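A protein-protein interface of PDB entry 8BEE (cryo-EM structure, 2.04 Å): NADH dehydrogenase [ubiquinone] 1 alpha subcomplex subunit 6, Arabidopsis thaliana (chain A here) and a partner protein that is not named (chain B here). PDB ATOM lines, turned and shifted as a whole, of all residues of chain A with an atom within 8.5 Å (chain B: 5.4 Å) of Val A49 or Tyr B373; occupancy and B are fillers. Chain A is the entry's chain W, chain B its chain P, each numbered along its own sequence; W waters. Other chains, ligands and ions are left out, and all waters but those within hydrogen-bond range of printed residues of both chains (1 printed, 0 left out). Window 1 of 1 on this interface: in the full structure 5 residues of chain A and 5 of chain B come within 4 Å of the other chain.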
ATOM      1  N   MET A  41     -20.990 -37.978  -2.280  1.00  0.00           N
ATOM      2  CA  MET A  41     -20.243 -36.861  -2.847  1.00  0.00           C
ATOM      3  C   MET A  41     -21.186 -35.824  -3.436  1.00  0.00           C
ATOM      4  O   MET A  41     -20.984 -34.617  -3.256  1.00  0.00           O
ATOM      5  CB  MET A  41     -19.269 -37.353  -3.918  1.00  0.00           C
ATOM      6  CG  MET A  41     -18.216 -38.328  -3.429  1.00  0.00           C
ATOM      7  SD  MET A  41     -16.753 -37.515  -2.770  1.00  0.00           S
ATOM      8  CE  MET A  41     -16.095 -36.739  -4.244  1.00  0.00           C
ATOM      9  N   ILE A  43     -24.443 -35.380  -2.581  1.00  0.00           N
ATOM     10  CA  ILE A  43     -25.324 -34.808  -1.564  1.00  0.00           C
ATOM     11  C   ILE A  43     -24.595 -33.745  -0.753  1.00  0.00           C
ATOM     12  O   ILE A  43     -25.145 -32.676  -0.466  1.00  0.00           O
ATOM     13  CB  ILE A  43     -25.892 -35.923  -0.663  1.00  0.00           C
ATOM     14  CG1 ILE A  43     -27.143 -36.531  -1.291  1.00  0.00           C
ATOM     15  CG2 ILE A  43     -26.230 -35.383   0.713  1.00  0.00           C
ATOM     16  CD1 ILE A  43     -27.646 -37.767  -0.581  1.00  0.00           C
ATOM     17  N   TYR A  44     -23.348 -34.012  -0.379  1.00  0.00           N
ATOM     18  CA  TYR A  44     -22.571 -33.095   0.443  1.00  0.00           C
ATOM     19  C   TYR A  44     -21.700 -32.139  -0.368  1.00  0.00           C
ATOM     20  O   TYR A  44     -20.972 -31.341   0.230  1.00  0.00           O
ATOM     21  CB  TYR A  44     -21.693 -33.880   1.428  1.00  0.00           C
ATOM     22  CG  TYR A  44     -22.458 -34.736   2.421  1.00  0.00           C
ATOM     23  CD1 TYR A  44     -23.038 -35.938   2.036  1.00  0.00           C
ATOM     24  CD2 TYR A  44     -22.584 -34.349   3.749  1.00  0.00           C
ATOM     25  CE1 TYR A  44     -23.733 -36.716   2.936  1.00  0.00           C
ATOM     26  CE2 TYR A  44     -23.275 -35.126   4.657  1.00  0.00           C
ATOM     27  CZ  TYR A  44     -23.848 -36.306   4.248  1.00  0.00           C
ATOM     28  OH  TYR A  44     -24.535 -37.084   5.148  1.00  0.00           O
ATOM     29  N   ASN A  45     -21.752 -32.196  -1.700  1.00  0.00           N
ATOM     30  CA  ASN A  45     -20.964 -31.318  -2.571  1.00  0.00           C
ATOM     31  C   ASN A  45     -19.477 -31.390  -2.230  1.00  0.00           C
ATOM     32  O   ASN A  45     -18.854 -30.413  -1.814  1.00  0.00           O
ATOM     33  CB  ASN A  45     -21.467 -29.874  -2.501  1.00  0.00           C
ATOM     34  CG  ASN A  45     -22.970 -29.782  -2.571  1.00  0.00           C
ATOM     35  OD1 ASN A  45     -23.556 -29.884  -3.645  1.00  0.00           O
ATOM     36  ND2 ASN A  45     -23.607 -29.591  -1.422  1.00  0.00           N
ATOM     37  N   LEU A  46     -18.891 -32.546  -2.453  1.00  0.00           N
ATOM     38  CA  LEU A  46     -17.512 -32.695  -1.958  1.00  0.00           C
ATOM     39  C   LEU A  46     -16.493 -32.677  -3.070  1.00  0.00           C
ATOM     40  O   LEU A  46     -15.349 -32.782  -2.730  1.00  0.00           O
ATOM     41  CB  LEU A  46     -17.470 -33.979  -1.119  1.00  0.00           C
ATOM     42  CG  LEU A  46     -18.226 -33.929   0.204  1.00  0.00           C
ATOM     43  CD1 LEU A  46     -18.276 -35.298   0.851  1.00  0.00           C
ATOM     44  CD2 LEU A  46     -17.617 -32.919   1.145  1.00  0.00           C
ATOM     45  N   GLN A  47     -16.930 -32.418  -4.317  1.00  0.00           N
ATOM     46  CA  GLN A  47     -16.043 -32.541  -5.471  1.00  0.00           C
ATOM     47  C   GLN A  47     -14.734 -31.794  -5.251  1.00  0.00           C
ATOM     48  O   GLN A  47     -13.657 -32.310  -5.569  1.00  0.00           O
ATOM     49  CB  GLN A  47     -16.730 -32.044  -6.748  1.00  0.00           C
ATOM     50  CG  GLN A  47     -18.060 -32.713  -7.160  1.00  0.00           C
ATOM     51  CD  GLN A  47     -19.197 -32.598  -6.154  1.00  0.00           C
ATOM     52  OE1 GLN A  47     -19.013 -32.157  -5.023  1.00  0.00           O
ATOM     53  NE2 GLN A  47     -20.392 -32.998  -6.577  1.00  0.00           N
ATOM     54  N   ASP A  48     -14.800 -30.589  -4.695  1.00  0.00           N
ATOM     55  CA  ASP A  48     -13.612 -29.778  -4.476  1.00  0.00           C
ATOM     56  C   ASP A  48     -13.125 -29.841  -3.035  1.00  0.00           C
ATOM     57  O   ASP A  48     -12.378 -28.958  -2.604  1.00  0.00           O
ATOM     58  CB  ASP A  48     -13.886 -28.331  -4.884  1.00  0.00           C
ATOM     59  CG  ASP A  48     -14.506 -28.226  -6.262  1.00  0.00           C
ATOM     60  OD1 ASP A  48     -14.377 -29.191  -7.046  1.00  0.00           O
ATOM     61  OD2 ASP A  48     -15.124 -27.183  -6.562  1.00  0.00           O
ATOM     62  N   VAL A  49     -13.518 -30.894  -2.295  1.00  0.00           N
ATOM     63  CA  VAL A  49     -13.166 -30.979  -0.842  1.00  0.00           C
ATOM     64  C   VAL A  49     -12.338 -32.223  -0.514  1.00  0.00           C
ATOM     65  O   VAL A  49     -11.485 -32.102   0.334  1.00  0.00           O
ATOM     66  CB  VAL A  49     -14.442 -30.982   0.010  1.00  0.00           C
ATOM     67  CG1 VAL A  49     -14.160 -31.210   1.486  1.00  0.00           C
ATOM     68  CG2 VAL A  49     -15.261 -29.718  -0.174  1.00  0.00           C
ATOM     69  N   VAL A  50     -12.609 -33.338  -1.178  1.00  0.00           N
ATOM     70  CA  VAL A  50     -11.967 -34.634  -0.829  1.00  0.00           C
ATOM     71  C   VAL A  50     -12.228 -35.630  -1.945  1.00  0.00           C
ATOM     72  O   VAL A  50     -13.234 -35.528  -2.601  1.00  0.00           O
ATOM     73  CB  VAL A  50     -12.551 -35.183   0.492  1.00  0.00           C
ATOM     74  CG1 VAL A  50     -13.922 -35.805   0.299  1.00  0.00           C
ATOM     75  CG2 VAL A  50     -11.615 -36.163   1.177  1.00  0.00           C
ATOM     76  N   ALA A  51     -11.291 -36.546  -2.167  1.00  0.00           N
ATOM     77  CA  ALA A  51     -11.394 -37.574  -3.189  1.00  0.00           C
ATOM     78  C   ALA A  51     -12.270 -38.730  -2.711  1.00  0.00           C
ATOM     79  O   ALA A  51     -12.322 -39.022  -1.513  1.00  0.00           O
ATOM     80  CB  ALA A  51     -10.012 -38.103  -3.551  1.00  0.00           C
ATOM     81  N   PRO A  52     -12.968 -39.402  -3.633  1.00  0.00           N
ATOM     82  CA  PRO A  52     -13.771 -40.571  -3.233  1.00  0.00           C
ATOM     83  C   PRO A  52     -12.956 -41.676  -2.586  1.00  0.00           C
ATOM     84  O   PRO A  52     -13.465 -42.372  -1.699  1.00  0.00           O
ATOM     85  CB  PRO A  52     -14.399 -41.030  -4.557  1.00  0.00           C
ATOM     86  CG  PRO A  52     -14.419 -39.811  -5.401  1.00  0.00           C
ATOM     87  CD  PRO A  52     -13.190 -39.035  -5.041  1.00  0.00           C
ATOM     88  N   GLN A  54     -10.520 -41.432  -0.526  1.00  0.00           N
ATOM     89  CA  GLN A  54     -10.354 -41.152   0.894  1.00  0.00           C
ATOM     90  C   GLN A  54     -11.562 -41.622   1.696  1.00  0.00           C
ATOM     91  O   GLN A  54     -11.411 -42.081   2.831  1.00  0.00           O
ATOM     92  CB  GLN A  54     -10.105 -39.659   1.102  1.00  0.00           C
ATOM     93  CG  GLN A  54      -8.837 -39.163   0.431  1.00  0.00           C
ATOM     94  CD  GLN A  54      -8.137 -38.080   1.226  1.00  0.00           C
ATOM     95  OE1 GLN A  54      -8.315 -36.892   0.967  1.00  0.00           O
ATOM     96  NE2 GLN A  54      -7.333 -38.489   2.201  1.00  0.00           N
ATOM     97  N   GLN A  95     -25.747 -32.000   6.674  1.00  0.00           N
ATOM     98  CA  GLN A  95     -24.529 -31.305   6.190  1.00  0.00           C
ATOM     99  C   GLN A  95     -23.841 -30.414   7.227  1.00  0.00           C
ATOM    100  O   GLN A  95     -24.515 -29.607   7.819  1.00  0.00           O
ATOM    101  CB  GLN A  95     -24.959 -30.434   5.040  1.00  0.00           C
ATOM    102  CG  GLN A  95     -25.224 -31.218   3.755  1.00  0.00           C
ATOM    103  CD  GLN A  95     -26.657 -31.112   3.299  1.00  0.00           C
ATOM    104  OE1 GLN A  95     -27.527 -30.633   4.024  1.00  0.00           O
ATOM    105  NE2 GLN A  95     -26.921 -31.560   2.083  1.00  0.00           N
ATOM    106  N   ARG A  96     -22.558 -30.604   7.491  1.00  0.00           N
ATOM    107  CA  ARG A  96     -21.739 -29.641   8.253  1.00  0.00           C
ATOM    108  C   ARG A  96     -20.729 -29.215   7.177  1.00  0.00           C
ATOM    109  O   ARG A  96     -21.140 -29.063   6.037  1.00  0.00           O
ATOM    110  CB  ARG A  96     -21.160 -30.173   9.572  1.00  0.00           C
ATOM    111  CG  ARG A  96     -22.210 -30.578  10.581  1.00  0.00           C
ATOM    112  CD  ARG A  96     -22.973 -29.329  10.954  1.00  0.00           C
ATOM    113  NE  ARG A  96     -22.230 -28.238  11.571  1.00  0.00           N
ATOM    114  CZ  ARG A  96     -21.907 -28.150  12.858  1.00  0.00           C
ATOM    115  NH1 ARG A  96     -22.235 -29.105  13.711  1.00  0.00           N
ATOM    116  NH2 ARG A  96     -21.255 -27.090  13.293  1.00  0.00           N
ATOM    117  N   HIS A  97     -19.505 -28.891   7.559  1.00  0.00           N
ATOM    118  CA  HIS A  97     -18.564 -28.548   6.471  1.00  0.00           C
ATOM    119  C   HIS A  97     -17.566 -29.686   6.356  1.00  0.00           C
ATOM    120  O   HIS A  97     -17.747 -30.559   5.498  1.00  0.00           O
ATOM    121  CB  HIS A  97     -17.901 -27.191   6.737  1.00  0.00           C
ATOM    122  CG  HIS A  97     -18.557 -26.059   6.020  1.00  0.00           C
ATOM    123  ND1 HIS A  97     -17.852 -24.956   5.581  1.00  0.00           N
ATOM    124  CD2 HIS A  97     -19.840 -25.861   5.651  1.00  0.00           C
ATOM    125  CE1 HIS A  97     -18.676 -24.122   4.980  1.00  0.00           C
ATOM    126  NE2 HIS A  97     -19.902 -24.654   5.011  1.00  0.00           N
ATOM    127  N   HIS A  98     -16.635 -29.745   7.291  1.00  0.00           N
ATOM    128  CA  HIS A  98     -15.545 -30.721   7.170  1.00  0.00           C
ATOM    129  C   HIS A  98     -15.914 -32.020   7.846  1.00  0.00           C
ATOM    130  O   HIS A  98     -15.029 -32.794   8.126  1.00  0.00           O
ATOM    131  CB  HIS A  98     -14.471 -30.060   7.941  1.00  0.00           C
ATOM    132  CG  HIS A  98     -13.797 -29.065   7.061  1.00  0.00           C
ATOM    133  ND1 HIS A  98     -13.067 -29.463   5.977  1.00  0.00           N
ATOM    134  CD2 HIS A  98     -13.797 -27.719   7.051  1.00  0.00           C
ATOM    135  CE1 HIS A  98     -12.595 -28.415   5.355  1.00  0.00           C
ATOM    136  NE2 HIS A  98     -13.023 -27.333   5.992  1.00  0.00           N
ATOM    137  N   ILE A  99     -17.190 -32.255   8.039  1.00  0.00           N
ATOM    138  CA  ILE A  99     -17.596 -33.420   8.874  1.00  0.00           C
ATOM    139  C   ILE A  99     -18.764 -34.158   8.226  1.00  0.00           C
ATOM    140  O   ILE A  99     -19.756 -33.497   7.978  1.00  0.00           O
ATOM    141  CB  ILE A  99     -18.008 -32.906  10.272  1.00  0.00           C
ATOM    142  CG1 ILE A  99     -16.815 -32.439  11.108  1.00  0.00           C
ATOM    143  CG2 ILE A  99     -18.825 -33.949  11.017  1.00  0.00           C
ATOM    144  CD1 ILE A  99     -17.202 -31.578  12.286  1.00  0.00           C
ATOM    145  N   ILE A 100     -18.653 -35.460   7.990  1.00  0.00           N
ATOM    146  CA  ILE A 100     -19.835 -36.277   7.556  1.00  0.00           C
ATOM    147  C   ILE A 100     -20.124 -37.254   8.706  1.00  0.00           C
ATOM    148  O   ILE A 100     -19.199 -37.938   9.086  1.00  0.00           O
ATOM    149  CB  ILE A 100     -19.595 -37.090   6.277  1.00  0.00           C
ATOM    150  CG1 ILE A 100     -19.233 -36.217   5.074  1.00  0.00           C
ATOM    151  CG2 ILE A 100     -20.810 -37.941   5.970  1.00  0.00           C
ATOM    152  CD1 ILE A 100     -18.602 -37.005   3.962  1.00  0.00           C
ATOM    153  N   VAL A 104     -14.312 -36.730  10.161  1.00  0.00           N
ATOM    154  CA  VAL A 104     -13.826 -35.424   9.712  1.00  0.00           C
ATOM    155  C   VAL A 104     -13.443 -35.641   8.246  1.00  0.00           C
ATOM    156  O   VAL A 104     -12.589 -36.456   8.007  1.00  0.00           O
ATOM    157  CB  VAL A 104     -12.566 -34.986  10.468  1.00  0.00           C
ATOM    158  CG1 VAL A 104     -12.275 -33.512  10.237  1.00  0.00           C
ATOM    159  CG2 VAL A 104     -12.677 -35.273  11.960  1.00  0.00           C
ATOM    160  N   VAL A 105     -14.120 -34.969   7.338  1.00  0.00           N
ATOM    161  CA  VAL A 105     -13.861 -35.154   5.869  1.00  0.00           C
ATOM    162  C   VAL A 105     -13.101 -33.930   5.385  1.00  0.00           C
ATOM    163  O   VAL A 105     -12.986 -32.966   6.123  1.00  0.00           O
ATOM    164  CB  VAL A 105     -15.110 -35.303   4.984  1.00  0.00           C
ATOM    165  CG1 VAL A 105     -15.756 -33.988   4.574  1.00  0.00           C
ATOM    166  CG2 VAL A 105     -14.893 -36.219   3.792  1.00  0.00           C
ATOM    167  N   GLY A 106     -12.683 -33.955   4.124  1.00  0.00           N
ATOM    168  CA  GLY A 106     -11.808 -32.859   3.693  1.00  0.00           C
ATOM    169  C   GLY A 106     -10.646 -32.738   4.652  1.00  0.00           C
ATOM    170  O   GLY A 106      -9.817 -31.842   4.421  1.00  0.00           O
ATOM    171  N   TYR B 257     -11.670 -15.714   1.880  1.00  0.00           N
ATOM    172  CA  TYR B 257     -12.826 -16.159   2.648  1.00  0.00           C
ATOM    173  C   TYR B 257     -13.059 -15.240   3.842  1.00  0.00           C
ATOM    174  O   TYR B 257     -12.133 -14.942   4.601  1.00  0.00           O
ATOM    175  CB  TYR B 257     -12.601 -17.595   3.117  1.00  0.00           C
ATOM    176  CG  TYR B 257     -13.839 -18.338   3.565  1.00  0.00           C
ATOM    177  CD1 TYR B 257     -15.103 -17.982   3.115  1.00  0.00           C
ATOM    178  CD2 TYR B 257     -13.736 -19.396   4.456  1.00  0.00           C
ATOM    179  CE1 TYR B 257     -16.233 -18.673   3.539  1.00  0.00           C
ATOM    180  CE2 TYR B 257     -14.848 -20.089   4.880  1.00  0.00           C
ATOM    181  CZ  TYR B 257     -16.093 -19.727   4.422  1.00  0.00           C
ATOM    182  OH  TYR B 257     -17.194 -20.429   4.856  1.00  0.00           O
ATOM    183  N   HIS B 368      -8.264 -20.296   3.838  1.00  0.00           N
ATOM    184  CA  HIS B 368      -8.976 -21.338   3.117  1.00  0.00           C
ATOM    185  C   HIS B 368      -9.030 -21.018   1.626  1.00  0.00           C
ATOM    186  O   HIS B 368      -9.137 -19.857   1.222  1.00  0.00           O
ATOM    187  CB  HIS B 368     -10.391 -21.492   3.680  1.00  0.00           C
ATOM    188  CG  HIS B 368     -11.019 -22.826   3.412  1.00  0.00           C
ATOM    189  ND1 HIS B 368     -11.026 -23.414   2.166  1.00  0.00           N
ATOM    190  CD2 HIS B 368     -11.656 -23.690   4.237  1.00  0.00           C
ATOM    191  CE1 HIS B 368     -11.644 -24.579   2.233  1.00  0.00           C
ATOM    192  NE2 HIS B 368     -12.036 -24.770   3.479  1.00  0.00           N
ATOM    193  N   LEU B 370     -10.747 -20.907  -2.072  1.00  0.00           N
ATOM    194  CA  LEU B 370     -12.091 -20.443  -2.404  1.00  0.00           C
ATOM    195  C   LEU B 370     -12.987 -21.584  -2.874  1.00  0.00           C
ATOM    196  O   LEU B 370     -14.152 -21.678  -2.470  1.00  0.00           O
ATOM    197  CB  LEU B 370     -12.021 -19.345  -3.467  1.00  0.00           C
ATOM    198  CG  LEU B 370     -11.485 -17.984  -3.023  1.00  0.00           C
ATOM    199  CD1 LEU B 370     -12.101 -16.879  -3.860  1.00  0.00           C
ATOM    200  CD2 LEU B 370     -11.750 -17.749  -1.546  1.00  0.00           C
ATOM    201  N   LYS B 371     -12.469 -22.449  -3.745  1.00  0.00           N
ATOM    202  CA  LYS B 371     -13.295 -23.479  -4.367  1.00  0.00           C
ATOM    203  C   LYS B 371     -13.921 -24.396  -3.328  1.00  0.00           C
ATOM    204  O   LYS B 371     -13.272 -24.800  -2.362  1.00  0.00           O
ATOM    205  CB  LYS B 371     -12.465 -24.299  -5.351  1.00  0.00           C
ATOM    206  CG  LYS B 371     -12.518 -23.795  -6.775  1.00  0.00           C
ATOM    207  CD  LYS B 371     -11.261 -24.180  -7.539  1.00  0.00           C
ATOM    208  CE  LYS B 371     -11.564 -24.436  -9.006  1.00  0.00           C
ATOM    209  NZ  LYS B 371     -10.363 -24.905  -9.752  1.00  0.00           N
ATOM    210  N   GLY B 372     -15.193 -24.707  -3.530  1.00  0.00           N
ATOM    211  CA  GLY B 372     -15.913 -25.601  -2.641  1.00  0.00           C
ATOM    212  C   GLY B 372     -16.697 -24.833  -1.586  1.00  0.00           C
ATOM    213  O   GLY B 372     -17.694 -24.183  -1.892  1.00  0.00           O
ATOM    214  N   TYR B 373     -16.238 -24.918  -0.340  1.00  0.00           N
ATOM    215  CA  TYR B 373     -17.019 -24.407   0.786  1.00  0.00           C
ATOM    216  C   TYR B 373     -17.195 -22.893   0.766  1.00  0.00           C
ATOM    217  O   TYR B 373     -18.330 -22.429   0.974  1.00  0.00           O
ATOM    218  CB  TYR B 373     -16.378 -24.908   2.080  1.00  0.00           C
ATOM    219  CG  TYR B 373     -16.821 -26.304   2.391  1.00  0.00           C
ATOM    220  CD1 TYR B 373     -17.952 -26.831   1.787  1.00  0.00           C
ATOM    221  CD2 TYR B 373     -16.057 -27.132   3.186  1.00  0.00           C
ATOM    222  CE1 TYR B 373     -18.356 -28.112   2.034  1.00  0.00           C
ATOM    223  CE2 TYR B 373     -16.444 -28.421   3.427  1.00  0.00           C
ATOM    224  CZ  TYR B 373     -17.600 -28.908   2.850  1.00  0.00           C
ATOM    225  OH  TYR B 373     -18.002 -30.202   3.091  1.00  0.00           O
ATOM    226  N   PRO B 374     -16.160 -22.074   0.541  1.00  0.00           N
ATOM    227  CA  PRO B 374     -16.399 -20.621   0.476  1.00  0.00           C
ATOM    228  C   PRO B 374     -17.373 -20.198  -0.612  1.00  0.00           C
ATOM    229  O   PRO B 374     -18.057 -19.180  -0.446  1.00  0.00           O
ATOM    230  CB  PRO B 374     -14.995 -20.056   0.235  1.00  0.00           C
ATOM    231  CG  PRO B 374     -14.110 -21.028   0.904  1.00  0.00           C
ATOM    232  CD  PRO B 374     -14.716 -22.366   0.585  1.00  0.00           C
ATOM    233  N   VAL B 375     -17.464 -20.937  -1.718  1.00  0.00           N
ATOM    234  CA  VAL B 375     -18.402 -20.614  -2.787  1.00  0.00           C
ATOM    235  C   VAL B 375     -19.642 -21.502  -2.744  1.00  0.00           C
ATOM    236  O   VAL B 375     -20.437 -21.496  -3.688  1.00  0.00           O
ATOM    237  CB  VAL B 375     -17.724 -20.696  -4.165  1.00  0.00           C
ATOM    238  CG1 VAL B 375     -16.657 -19.618  -4.302  1.00  0.00           C
ATOM    239  CG2 VAL B 375     -17.122 -22.072  -4.377  1.00  0.00           C
ATOM    240  N   GLU B 376     -19.806 -22.416  -1.808  1.00  0.00           N
ATOM    241  CA  GLU B 376     -21.043 -23.244  -1.694  1.00  0.00           C
ATOM    242  C   GLU B 376     -22.344 -22.412  -1.659  1.00  0.00           C
ATOM    243  O   GLU B 376     -23.359 -22.911  -2.109  1.00  0.00           O
ATOM    244  CB  GLU B 376     -20.990 -23.998  -0.392  1.00  0.00           C
ATOM    245  CG  GLU B 376     -22.044 -25.075  -0.229  1.00  0.00           C
ATOM    246  CD  GLU B 376     -22.101 -25.631   1.182  1.00  0.00           C
ATOM    247  OE1 GLU B 376     -21.427 -25.063   2.066  1.00  0.00           O
ATOM    248  OE2 GLU B 376     -22.820 -26.626   1.394  1.00  0.00           O
ATOM    249  N   PHE B 377     -22.327 -21.179  -1.196  1.00  0.00           N
ATOM    250  CA  PHE B 377     -23.572 -20.424  -1.256  1.00  0.00           C
ATOM    251  C   PHE B 377     -24.067 -20.237  -2.685  1.00  0.00           C
ATOM    252  O   PHE B 377     -25.251 -19.947  -2.884  1.00  0.00           O
ATOM    253  CB  PHE B 377     -23.401 -19.064  -0.581  1.00  0.00           C
ATOM    254  CG  PHE B 377     -22.535 -18.112  -1.349  1.00  0.00           C
ATOM    255  CD1 PHE B 377     -21.157 -18.199  -1.276  1.00  0.00           C
ATOM    256  CD2 PHE B 377     -23.099 -17.127  -2.143  1.00  0.00           C
ATOM    257  CE1 PHE B 377     -20.356 -17.324  -1.983  1.00  0.00           C
ATOM    258  CE2 PHE B 377     -22.304 -16.253  -2.850  1.00  0.00           C
ATOM    259  CZ  PHE B 377     -20.932 -16.353  -2.769  1.00  0.00           C
HETATM  260  O   HOH W   1     -13.592 -24.705   6.371  1.00  0.00           O
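Of the 10 printed residues of chain B, 5 touch a printed residue of chain A.
Hydrophobic or aromatic side chains of chain B that line the printed part of chain A: Tyr B257, His B368 and Tyr B373.
Hydrophobic or aromatic side chains of chain A within 4 Å of the printed part of chain B: Leu A46, Val A49, His A97 and His A98.
Among the printed residues, 7 pairs touch across the chains.
Among the printed residues, no Asp or Glu carboxylate lies within 4 Å of a Lys or Arg side-chain nitrogen of the other chain.
Water W1 bridges a ring nitrogen (NE2) of His A98 (2.7 Å) and a ring nitrogen (NE2) of His B368 (3.3 Å).
Leu A46 touches Tyr B373 (CD2 to OH, 3.4 Å).
OD2 of Asp A48 touches N of Gly B372, at 3.9 Å.
Val A49 touches Tyr B373 (CG2 to CZ, 3.9 Å).
Tyr B257 touches His A97.
His A98 touches His B368.
OH of Tyr B373 is in hydrogen-bond range of O of His A97.
OE1 of Glu B376 is in hydrogen-bond range of NE2 of His A97, at 3.3 Å.
N of Leu A46 is in hydrogen-bond range of O of Met A41.
The backbone carbonyl oxygen (O) of His A98 lies within hydrogen-bond range of the backbone NH (N) of Val A105 (2.5 Å).
Tyr A44 touches none of the printed residues of chain B.
Of the printed residues of chain B, Leu A46 touches Tyr B373 (3.4 Å).
Of the printed residues of chain B, Asp A48 touches Gly B372 (3.9 Å).
Of the printed residues of chain B, Val A49 touches Tyr B373.
Arg A96 touches none of the printed residues of chain B.
Printed residues of chain B within 4 Å of His A98: His B368 (3.7 Å).
Of the printed residues of chain A, Tyr B257 touches His A97 (3.98 Å).
Of chain A, only Leu A46 (3.4 Å), Val A49 (3.9 Å) and His A97 (2.4 Å) come within 4 Å of Tyr B373.
No residue of chain A comes within 4 Å of Pro B374.
Of the printed residues of chain A, Glu B376 touches His A97 (3.3 Å).
The nearest residue of chain B that does not touch Val A49 is Gly B372 (4.8 Å).
The nearest residue of chain A that does not touch Tyr B373 is His A98 (4.1 Å).
The nearest printed residue of chain A that does not touch His B368 is His A97 (6.2 Å).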
